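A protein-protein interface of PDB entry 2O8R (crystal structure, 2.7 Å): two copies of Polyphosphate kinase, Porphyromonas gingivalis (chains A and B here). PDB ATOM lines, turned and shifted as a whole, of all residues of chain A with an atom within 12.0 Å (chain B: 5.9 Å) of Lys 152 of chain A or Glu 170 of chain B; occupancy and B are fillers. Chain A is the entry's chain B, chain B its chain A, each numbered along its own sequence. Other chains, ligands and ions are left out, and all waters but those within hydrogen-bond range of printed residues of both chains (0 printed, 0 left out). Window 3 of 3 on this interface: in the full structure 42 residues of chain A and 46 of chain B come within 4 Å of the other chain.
Hydrophobic or aromatic side chains of chain B that line the printed part of chain A: Pro 222 and Tyr 224.
Hydrophobic or aromatic side chains of chain A within 4 Å of the printed part of chain B: Leu 149 and Val 153.
Among the printed residues, Asp or Glu carboxylates within 4 Å of a Lys or Arg side-chain nitrogen of the other chain: Lys 152 of chain A with Glu 170 of chain B.
Lys 152 of chain A touches five residues of chain B.
Of the printed residues of chain A, Glu 170 of chain B touches Lys 152.
No residue of chain A comes within 4 Å of Lys 169 of chain B.
No residue of chain A comes within 4 Å of Glu 172 of chain B.
No residue of chain A comes within 4 Å of Ala 176 of chain B.
Of chain A, only Ser 151 (3.6 Å) and Lys 152 (2.8 Å) come within 4 Å of Gly 223 of chain B.
Of the printed residues of chain A, Phe 221 of chain B touches Lys 152 (3.3 Å).
Of the printed residues of chain B, Arg 154 of chain A touches Val 220 (2.8 Å) and Pro 222 (3.4 Å).
Pro 150 of chain A touches none of the printed residues of chain B.
Phe 156 of chain A touches none of the printed residues of chain B.
The nearest residue of chain B that does not touch Lys 152 of chain A is Val 220 of chain B (4.5 Å).
The nearest residue of chain A that does not touch Glu 170 of chain B is Leu 149 of chain A (5.8 Å).
The nearest printed residue of chain A that does not touch Val 220 of chain B is Lys 152 of chain A (4.5 Å).
2 positions are printed for both chains.
The backbone carbonyl oxygen (O) of Lys 152 of chain A sits close to the backbone nitrogen (N) of Pro 222 of chain B (3.1 Å).
The side-chain amino group (NZ) of Lys 152 of chain A is in salt-bridge range of the side-chain carboxylate (OE1) of Glu 170 of chain B, at 3.9 Å.
O of Lys 152 of chain A lies within hydrogen-bond range of N of Gly 223 of chain B.
O of Val 220 of chain B sits at hydrogen-bond distance from N of Arg 154 of chain A (2.8 Å).
Tyr 224 of chain B touches Leu 149 of chain A (OH to CD2, 3.6 Å).
O of Ser 151 of chain A touches CG of Pro 222 of chain B, 3.4 Å away.
O of Ser 151 of chain A touches N of Gly 223 of chain B, 3.6 Å away.
C of Phe 221 of chain B touches O of Lys 152 of chain A, at 3.3 Å.
O of Lys 152 of chain A touches CD2 of Tyr 224 of chain B, 3.4 Å away.
Val 220 of chain B touches Val 153 of chain A (O to CA, 3.4 Å).
CA of Val 153 of chain A touches CD of Pro 222 of chain B, 3.9 Å away.
CB of Pro 222 of chain B touches NH2 of Arg 154 of chain A, 3.4 Å away.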
ATOM      1  N   MET A 146       8.754   1.577  17.128  1.00  0.00           N
ATOM      2  CA  MET A 146       9.940   2.344  17.482  1.00  0.00           C
ATOM      3  C   MET A 146      10.535   1.825  18.782  1.00  0.00           C
ATOM      4  O   MET A 146       9.859   1.828  19.811  1.00  0.00           O
ATOM      5  CB  MET A 146       9.575   3.812  17.672  1.00  0.00           C
ATOM      6  CG  MET A 146       8.694   4.392  16.588  1.00  0.00           C
ATOM      7  SD  MET A 146       7.675   5.899  17.272  1.00  0.00           S
ATOM      8  CE  MET A 146       6.088   4.995  17.998  1.00  0.00           C
ATOM      9  N   LEU A 147      11.787   1.372  18.736  1.00  0.00           N
ATOM     10  CA  LEU A 147      12.523   1.053  19.966  1.00  0.00           C
ATOM     11  C   LEU A 147      12.804   2.352  20.707  1.00  0.00           C
ATOM     12  O   LEU A 147      13.304   3.307  20.114  1.00  0.00           O
ATOM     13  CB  LEU A 147      13.855   0.345  19.669  1.00  0.00           C
ATOM     14  CG  LEU A 147      13.814  -0.885  18.766  1.00  0.00           C
ATOM     15  CD1 LEU A 147      15.200  -1.235  18.195  1.00  0.00           C
ATOM     16  CD2 LEU A 147      13.195  -2.062  19.482  1.00  0.00           C
ATOM     17  N   LEU A 148      12.467   2.389  21.991  1.00  0.00           N
ATOM     18  CA  LEU A 148      12.774   3.540  22.831  1.00  0.00           C
ATOM     19  C   LEU A 148      14.255   3.582  23.261  1.00  0.00           C
ATOM     20  O   LEU A 148      14.706   2.726  24.025  1.00  0.00           O
ATOM     21  CB  LEU A 148      11.850   3.560  24.050  1.00  0.00           C
ATOM     22  CG  LEU A 148      10.386   3.912  23.777  1.00  0.00           C
ATOM     23  CD1 LEU A 148       9.539   3.834  25.046  1.00  0.00           C
ATOM     24  CD2 LEU A 148      10.286   5.290  23.176  1.00  0.00           C
ATOM     25  N   LEU A 149      14.999   4.571  22.753  1.00  0.00           N
ATOM     26  CA  LEU A 149      16.390   4.838  23.154  1.00  0.00           C
ATOM     27  C   LEU A 149      16.542   6.286  23.632  1.00  0.00           C
ATOM     28  O   LEU A 149      17.165   7.101  22.951  1.00  0.00           O
ATOM     29  CB  LEU A 149      17.349   4.581  21.996  1.00  0.00           C
ATOM     30  CG  LEU A 149      17.904   3.171  21.804  1.00  0.00           C
ATOM     31  CD1 LEU A 149      16.828   2.201  21.344  1.00  0.00           C
ATOM     32  CD2 LEU A 149      19.064   3.195  20.806  1.00  0.00           C
ATOM     33  N   PRO A 150      16.037   6.577  24.843  1.00  0.00           N
ATOM     34  CA  PRO A 150      15.603   7.867  25.382  1.00  0.00           C
ATOM     35  C   PRO A 150      16.442   9.092  25.008  1.00  0.00           C
ATOM     36  O   PRO A 150      15.876  10.121  24.636  1.00  0.00           O
ATOM     37  CB  PRO A 150      15.633   7.643  26.901  1.00  0.00           C
ATOM     38  CG  PRO A 150      16.285   6.295  27.101  1.00  0.00           C
ATOM     39  CD  PRO A 150      15.953   5.535  25.874  1.00  0.00           C
ATOM     40  N   SER A 151      17.766   9.002  25.104  1.00  0.00           N
ATOM     41  CA  SER A 151      18.595  10.182  24.853  1.00  0.00           C
ATOM     42  C   SER A 151      19.311  10.169  23.496  1.00  0.00           C
ATOM     43  O   SER A 151      19.865  11.182  23.063  1.00  0.00           O
ATOM     44  CB  SER A 151      19.593  10.384  25.989  1.00  0.00           C
ATOM     45  OG  SER A 151      20.047  11.726  26.010  1.00  0.00           O
ATOM     46  N   LYS A 152      19.301   9.023  22.830  1.00  0.00           N
ATOM     47  CA  LYS A 152      19.911   8.911  21.523  1.00  0.00           C
ATOM     48  C   LYS A 152      18.950   9.404  20.453  1.00  0.00           C
ATOM     49  O   LYS A 152      19.341  10.131  19.536  1.00  0.00           O
ATOM     50  CB  LYS A 152      20.324   7.464  21.233  1.00  0.00           C
ATOM     51  CG  LYS A 152      21.788   7.154  21.536  1.00  0.00           C
ATOM     52  CD  LYS A 152      21.963   6.291  22.790  1.00  0.00           C
ATOM     53  CE  LYS A 152      21.956   4.805  22.451  1.00  0.00           C
ATOM     54  NZ  LYS A 152      22.211   3.938  23.635  1.00  0.00           N
ATOM     55  N   VAL A 153      17.690   8.998  20.572  1.00  0.00           N
ATOM     56  CA  VAL A 153      16.678   9.332  19.579  1.00  0.00           C
ATOM     57  C   VAL A 153      15.450   9.890  20.276  1.00  0.00           C
ATOM     58  O   VAL A 153      14.931   9.284  21.214  1.00  0.00           O
ATOM     59  CB  VAL A 153      16.340   8.113  18.649  1.00  0.00           C
ATOM     60  CG1 VAL A 153      16.417   6.821  19.416  1.00  0.00           C
ATOM     61  CG2 VAL A 153      14.968   8.270  17.950  1.00  0.00           C
ATOM     62  N   ARG A 154      15.016  11.060  19.808  1.00  0.00           N
ATOM     63  CA  ARG A 154      13.912  11.809  20.399  1.00  0.00           C
ATOM     64  C   ARG A 154      12.608  11.456  19.712  1.00  0.00           C
ATOM     65  O   ARG A 154      12.591  11.186  18.511  1.00  0.00           O
ATOM     66  CB  ARG A 154      14.187  13.290  20.216  1.00  0.00           C
ATOM     67  CG  ARG A 154      13.475  14.198  21.184  1.00  0.00           C
ATOM     68  CD  ARG A 154      13.959  15.634  20.996  1.00  0.00           C
ATOM     69  NE  ARG A 154      15.418  15.745  21.042  1.00  0.00           N
ATOM     70  CZ  ARG A 154      16.088  16.893  21.015  1.00  0.00           C
ATOM     71  NH1 ARG A 154      15.440  18.049  20.937  1.00  0.00           N
ATOM     72  NH2 ARG A 154      17.414  16.890  21.062  1.00  0.00           N
ATOM     73  N   THR A 155      11.511  11.458  20.462  1.00  0.00           N
ATOM     74  CA  THR A 155      10.219  11.115  19.880  1.00  0.00           C
ATOM     75  C   THR A 155       9.010  11.722  20.594  1.00  0.00           C
ATOM     76  O   THR A 155       9.035  11.958  21.802  1.00  0.00           O
ATOM     77  CB  THR A 155      10.038   9.590  19.740  1.00  0.00           C
ATOM     78  OG1 THR A 155       8.856   9.325  18.974  1.00  0.00           O
ATOM     79  CG2 THR A 155       9.940   8.914  21.107  1.00  0.00           C
ATOM     80  N   PHE A 156       7.952  11.959  19.824  1.00  0.00           N
ATOM     81  CA  PHE A 156       6.764  12.620  20.315  1.00  0.00           C
ATOM     82  C   PHE A 156       5.668  11.620  20.654  1.00  0.00           C
ATOM     83  O   PHE A 156       5.529  10.589  20.000  1.00  0.00           O
ATOM     84  CB  PHE A 156       6.258  13.624  19.282  1.00  0.00           C
ATOM     85  CG  PHE A 156       5.228  14.583  19.818  1.00  0.00           C
ATOM     86  CD1 PHE A 156       5.614  15.781  20.405  1.00  0.00           C
ATOM     87  CD2 PHE A 156       3.868  14.291  19.735  1.00  0.00           C
ATOM     88  CE1 PHE A 156       4.658  16.669  20.903  1.00  0.00           C
ATOM     89  CE2 PHE A 156       2.906  15.174  20.237  1.00  0.00           C
ATOM     90  CZ  PHE A 156       3.296  16.359  20.819  1.00  0.00           C
ATOM     91  N   TYR A 177      16.404  -4.910  30.358  1.00  0.00           N
ATOM     92  CA  TYR A 177      15.294  -4.767  29.409  1.00  0.00           C
ATOM     93  C   TYR A 177      15.504  -3.721  28.309  1.00  0.00           C
ATOM     94  O   TYR A 177      15.857  -2.576  28.595  1.00  0.00           O
ATOM     95  CB  TYR A 177      14.018  -4.397  30.159  1.00  0.00           C
ATOM     96  CG  TYR A 177      13.353  -5.528  30.905  1.00  0.00           C
ATOM     97  CD1 TYR A 177      12.968  -6.685  30.247  1.00  0.00           C
ATOM     98  CD2 TYR A 177      13.069  -5.422  32.268  1.00  0.00           C
ATOM     99  CE1 TYR A 177      12.340  -7.719  30.924  1.00  0.00           C
ATOM    100  CE2 TYR A 177      12.442  -6.449  32.950  1.00  0.00           C
ATOM    101  CZ  TYR A 177      12.077  -7.598  32.269  1.00  0.00           C
ATOM    102  OH  TYR A 177      11.454  -8.636  32.921  1.00  0.00           O
ATOM    103  N   SER A 178      15.274  -4.119  27.057  1.00  0.00           N
ATOM    104  CA  SER A 178      15.004  -3.163  25.975  1.00  0.00           C
ATOM    105  C   SER A 178      13.591  -2.627  26.150  1.00  0.00           C
ATOM    106  O   SER A 178      12.752  -3.292  26.758  1.00  0.00           O
ATOM    107  CB  SER A 178      15.065  -3.867  24.622  1.00  0.00           C
ATOM    108  OG  SER A 178      16.395  -4.024  24.160  1.00  0.00           O
ATOM    109  N   TYR A 179      13.300  -1.443  25.625  1.00  0.00           N
ATOM    110  CA  TYR A 179      11.900  -0.993  25.586  1.00  0.00           C
ATOM    111  C   TYR A 179      11.488  -0.506  24.213  1.00  0.00           C
ATOM    112  O   TYR A 179      12.333  -0.118  23.414  1.00  0.00           O
ATOM    113  CB  TYR A 179      11.648   0.084  26.626  1.00  0.00           C
ATOM    114  CG  TYR A 179      11.753  -0.425  28.038  1.00  0.00           C
ATOM    115  CD1 TYR A 179      10.659  -0.989  28.671  1.00  0.00           C
ATOM    116  CD2 TYR A 179      12.954  -0.349  28.742  1.00  0.00           C
ATOM    117  CE1 TYR A 179      10.750  -1.456  29.968  1.00  0.00           C
ATOM    118  CE2 TYR A 179      13.058  -0.818  30.044  1.00  0.00           C
ATOM    119  CZ  TYR A 179      11.946  -1.367  30.656  1.00  0.00           C
ATOM    120  OH  TYR A 179      12.026  -1.840  31.953  1.00  0.00           O
ATOM    121  N   TYR A 224      13.020 -10.844  20.032  1.00  0.00           N
ATOM    122  CA  TYR A 224      12.888 -10.676  21.479  1.00  0.00           C
ATOM    123  C   TYR A 224      11.934 -11.708  22.038  1.00  0.00           C
ATOM    124  O   TYR A 224      11.087 -12.235  21.314  1.00  0.00           O
ATOM    125  CB  TYR A 224      12.334  -9.275  21.821  1.00  0.00           C
ATOM    126  CG  TYR A 224      13.147  -8.120  21.262  1.00  0.00           C
ATOM    127  CD1 TYR A 224      13.012  -7.716  19.928  1.00  0.00           C
ATOM    128  CD2 TYR A 224      14.048  -7.429  22.066  1.00  0.00           C
ATOM    129  CE1 TYR A 224      13.761  -6.667  19.416  1.00  0.00           C
ATOM    130  CE2 TYR A 224      14.797  -6.375  21.565  1.00  0.00           C
ATOM    131  CZ  TYR A 224      14.651  -6.002  20.242  1.00  0.00           C
ATOM    132  OH  TYR A 224      15.401  -4.961  19.750  1.00  0.00           O
ATOM    133  N   ARG A 281       9.501   5.755  33.713  1.00  0.00           N
ATOM    134  CA  ARG A 281      10.703   6.592  33.688  1.00  0.00           C
ATOM    135  C   ARG A 281      11.416   6.548  32.334  1.00  0.00           C
ATOM    136  O   ARG A 281      12.204   7.434  32.004  1.00  0.00           O
ATOM    137  CB  ARG A 281      11.668   6.167  34.799  1.00  0.00           C
ATOM    138  CG  ARG A 281      11.534   6.953  36.097  1.00  0.00           C
ATOM    139  CD  ARG A 281      12.326   6.288  37.219  1.00  0.00           C
ATOM    140  NE  ARG A 281      11.484   5.475  38.101  1.00  0.00           N
ATOM    141  CZ  ARG A 281      11.811   4.267  38.558  1.00  0.00           C
ATOM    142  NH1 ARG A 281      12.962   3.703  38.199  1.00  0.00           N
ATOM    143  NH2 ARG A 281      10.977   3.613  39.360  1.00  0.00           N
ATOM    144  N   TYR A 282      11.123   5.521  31.545  1.00  0.00           N
ATOM    145  CA  TYR A 282      11.710   5.387  30.225  1.00  0.00           C
ATOM    146  C   TYR A 282      11.022   6.309  29.223  1.00  0.00           C
ATOM    147  O   TYR A 282      11.346   6.292  28.035  1.00  0.00           O
ATOM    148  CB  TYR A 282      11.618   3.941  29.755  1.00  0.00           C
ATOM    149  CG  TYR A 282      12.945   3.391  29.343  1.00  0.00           C
ATOM    150  CD1 TYR A 282      13.300   3.312  28.001  1.00  0.00           C
ATOM    151  CD2 TYR A 282      13.858   2.965  30.300  1.00  0.00           C
ATOM    152  CE1 TYR A 282      14.531   2.812  27.619  1.00  0.00           C
ATOM    153  CE2 TYR A 282      15.092   2.463  29.932  1.00  0.00           C
ATOM    154  CZ  TYR A 282      15.426   2.390  28.592  1.00  0.00           C
ATOM    155  OH  TYR A 282      16.657   1.887  28.236  1.00  0.00           O
ATOM    156  N   ILE A 283      10.064   7.096  29.712  1.00  0.00           N
ATOM    157  CA  ILE A 283       9.349   8.085  28.902  1.00  0.00           C
ATOM    158  C   ILE A 283       9.020   9.332  29.718  1.00  0.00           C
ATOM    159  O   ILE A 283       9.175   9.347  30.940  1.00  0.00           O
ATOM    160  CB  ILE A 283       8.045   7.509  28.292  1.00  0.00           C
ATOM    161  CG1 ILE A 283       7.468   6.417  29.206  1.00  0.00           C
ATOM    162  CG2 ILE A 283       8.305   6.995  26.879  1.00  0.00           C
ATOM    163  CD1 ILE A 283       6.110   5.883  28.807  1.00  0.00           C
ATOM    164  N   LEU B 168      23.115   6.593  10.432  1.00  0.00           N
ATOM    165  CA  LEU B 168      23.599   7.216  11.662  1.00  0.00           C
ATOM    166  C   LEU B 168      24.928   6.653  12.190  1.00  0.00           C
ATOM    167  O   LEU B 168      25.139   5.436  12.190  1.00  0.00           O
ATOM    168  CB  LEU B 168      22.532   7.084  12.743  1.00  0.00           C
ATOM    169  CG  LEU B 168      21.163   7.648  12.387  1.00  0.00           C
ATOM    170  CD1 LEU B 168      20.074   6.947  13.188  1.00  0.00           C
ATOM    171  CD2 LEU B 168      21.127   9.156  12.604  1.00  0.00           C
ATOM    172  N   LYS B 169      25.808   7.547  12.648  1.00  0.00           N
ATOM    173  CA  LYS B 169      27.009   7.161  13.389  1.00  0.00           C
ATOM    174  C   LYS B 169      26.950   7.799  14.767  1.00  0.00           C
ATOM    175  O   LYS B 169      26.660   8.986  14.889  1.00  0.00           O
ATOM    176  CB  LYS B 169      28.267   7.594  12.654  1.00  0.00           C
ATOM    177  CG  LYS B 169      29.509   6.828  13.061  1.00  0.00           C
ATOM    178  CD  LYS B 169      30.752   7.612  12.687  1.00  0.00           C
ATOM    179  CE  LYS B 169      31.885   7.345  13.654  1.00  0.00           C
ATOM    180  NZ  LYS B 169      32.813   8.513  13.763  1.00  0.00           N
ATOM    181  N   GLU B 170      27.239   7.010  15.800  1.00  0.00           N
ATOM    182  CA  GLU B 170      26.882   7.349  17.179  1.00  0.00           C
ATOM    183  C   GLU B 170      27.899   8.230  17.917  1.00  0.00           C
ATOM    184  O   GLU B 170      28.281   9.288  17.427  1.00  0.00           O
ATOM    185  CB  GLU B 170      26.644   6.057  17.951  1.00  0.00           C
ATOM    186  CG  GLU B 170      25.554   6.132  18.990  1.00  0.00           C
ATOM    187  CD  GLU B 170      25.225   4.768  19.545  1.00  0.00           C
ATOM    188  OE1 GLU B 170      24.673   4.702  20.663  1.00  0.00           O
ATOM    189  OE2 GLU B 170      25.527   3.762  18.862  1.00  0.00           O
ATOM    190  N   LYS B 171      28.312   7.799  19.107  1.00  0.00           N
ATOM    191  CA  LYS B 171      29.348   8.485  19.880  1.00  0.00           C
ATOM    192  C   LYS B 171      30.725   7.932  19.528  1.00  0.00           C
ATOM    193  O   LYS B 171      31.672   8.691  19.310  1.00  0.00           O
ATOM    194  CB  LYS B 171      29.094   8.331  21.387  1.00  0.00           C
ATOM    195  CG  LYS B 171      30.299   8.656  22.283  1.00  0.00           C
ATOM    196  CD  LYS B 171      30.660  10.138  22.243  1.00  0.00           C
ATOM    197  CE  LYS B 171      32.127  10.365  22.557  1.00  0.00           C
ATOM    198  NZ  LYS B 171      32.550  11.731  22.144  1.00  0.00           N
ATOM    199  N   GLU B 172      30.816   6.605  19.485  1.00  0.00           N
ATOM    200  CA  GLU B 172      32.049   5.896  19.152  1.00  0.00           C
ATOM    201  C   GLU B 172      32.433   6.064  17.683  1.00  0.00           C
ATOM    202  O   GLU B 172      31.591   5.940  16.787  1.00  0.00           O
ATOM    203  CB  GLU B 172      31.941   4.406  19.514  1.00  0.00           C
ATOM    204  CG  GLU B 172      30.604   3.744  19.170  1.00  0.00           C
ATOM    205  CD  GLU B 172      29.548   3.910  20.261  1.00  0.00           C
ATOM    206  OE1 GLU B 172      29.826   4.578  21.282  1.00  0.00           O
ATOM    207  OE2 GLU B 172      28.432   3.373  20.091  1.00  0.00           O
ATOM    208  N   ALA B 176      30.898   1.124  12.197  1.00  0.00           N
ATOM    209  CA  ALA B 176      29.574   0.510  12.218  1.00  0.00           C
ATOM    210  C   ALA B 176      28.475   1.563  12.147  1.00  0.00           C
ATOM    211  O   ALA B 176      28.366   2.431  13.016  1.00  0.00           O
ATOM    212  CB  ALA B 176      29.412  -0.363  13.460  1.00  0.00           C
ATOM    213  N   SER B 178      24.550   2.807  12.044  1.00  0.00           N
ATOM    214  CA  SER B 178      23.158   2.554  12.371  1.00  0.00           C
ATOM    215  C   SER B 178      22.266   3.027  11.221  1.00  0.00           C
ATOM    216  O   SER B 178      22.681   3.834  10.386  1.00  0.00           O
ATOM    217  CB  SER B 178      22.784   3.283  13.654  1.00  0.00           C
ATOM    218  OG  SER B 178      22.925   2.424  14.768  1.00  0.00           O
ATOM    219  N   VAL B 220      15.953  14.964  15.853  1.00  0.00           N
ATOM    220  CA  VAL B 220      15.268  13.679  15.942  1.00  0.00           C
ATOM    221  C   VAL B 220      16.237  12.630  16.487  1.00  0.00           C
ATOM    222  O   VAL B 220      15.858  11.737  17.256  1.00  0.00           O
ATOM    223  CB  VAL B 220      14.706  13.269  14.561  1.00  0.00           C
ATOM    224  CG1 VAL B 220      14.149  11.864  14.580  1.00  0.00           C
ATOM    225  CG2 VAL B 220      13.632  14.252  14.129  1.00  0.00           C
ATOM    226  N   PHE B 221      17.502  12.772  16.120  1.00  0.00           N
ATOM    227  CA  PHE B 221      18.523  11.856  16.595  1.00  0.00           C
ATOM    228  C   PHE B 221      19.637  12.600  17.337  1.00  0.00           C
ATOM    229  O   PHE B 221      20.755  12.710  16.829  1.00  0.00           O
ATOM    230  CB  PHE B 221      19.096  11.076  15.412  1.00  0.00           C
ATOM    231  CG  PHE B 221      18.056  10.358  14.591  1.00  0.00           C
ATOM    232  CD1 PHE B 221      17.594   9.105  14.977  1.00  0.00           C
ATOM    233  CD2 PHE B 221      17.547  10.931  13.430  1.00  0.00           C
ATOM    234  CE1 PHE B 221      16.639   8.436  14.218  1.00  0.00           C
ATOM    235  CE2 PHE B 221      16.601  10.270  12.669  1.00  0.00           C
ATOM    236  CZ  PHE B 221      16.141   9.017  13.068  1.00  0.00           C
ATOM    237  N   PRO B 222      19.340  13.115  18.545  1.00  0.00           N
ATOM    238  CA  PRO B 222      20.325  13.926  19.257  1.00  0.00           C
ATOM    239  C   PRO B 222      21.629  13.184  19.577  1.00  0.00           C
ATOM    240  O   PRO B 222      22.706  13.770  19.499  1.00  0.00           O
ATOM    241  CB  PRO B 222      19.596  14.304  20.548  1.00  0.00           C
ATOM    242  CG  PRO B 222      18.541  13.273  20.704  1.00  0.00           C
ATOM    243  CD  PRO B 222      18.095  12.983  19.323  1.00  0.00           C
ATOM    244  N   GLY B 223      21.534  11.903  19.910  1.00  0.00           N
ATOM    245  CA  GLY B 223      22.712  11.125  20.246  1.00  0.00           C
ATOM    246  C   GLY B 223      23.437  10.493  19.073  1.00  0.00           C
ATOM    247  O   GLY B 223      24.116   9.476  19.241  1.00  0.00           O
ATOM    248  N   TYR B 224      23.303  11.084  17.889  1.00  0.00           N
ATOM    249  CA  TYR B 224      23.989  10.581  16.697  1.00  0.00           C
ATOM    250  C   TYR B 224      24.479  11.713  15.832  1.00  0.00           C
ATOM    251  O   TYR B 224      23.977  12.833  15.913  1.00  0.00           O
ATOM    252  CB  TYR B 224      23.059   9.742  15.822  1.00  0.00           C
ATOM    253  CG  TYR B 224      22.439   8.547  16.483  1.00  0.00           C
ATOM    254  CD1 TYR B 224      23.033   7.291  16.393  1.00  0.00           C
ATOM    255  CD2 TYR B 224      21.242   8.664  17.178  1.00  0.00           C
ATOM    256  CE1 TYR B 224      22.458   6.189  16.994  1.00  0.00           C
ATOM    257  CE2 TYR B 224      20.658   7.566  17.780  1.00  0.00           C
ATOM    258  CZ  TYR B 224      21.268   6.330  17.688  1.00  0.00           C
ATOM    259  OH  TYR B 224      20.678   5.243  18.292  1.00  0.00           O
ATOM    260  N   GLU B 225      25.447  11.393  14.982  1.00  0.00           N
ATOM    261  CA  GLU B 225      25.872  12.264  13.903  1.00  0.00           C
ATOM    262  C   GLU B 225      25.138  11.786  12.647  1.00  0.00           C
ATOM    263  O   GLU B 225      25.411  10.696  12.142  1.00  0.00           O
ATOM    264  CB  GLU B 225      27.390  12.169  13.719  1.00  0.00           C
ATOM    265  CG  GLU B 225      28.061  13.451  13.267  1.00  0.00           C
ATOM    266  CD  GLU B 225      28.004  14.543  14.320  1.00  0.00           C
ATOM    267  OE1 GLU B 225      27.801  15.724  13.952  1.00  0.00           O
ATOM    268  OE2 GLU B 225      28.156  14.220  15.519  1.00  0.00           O
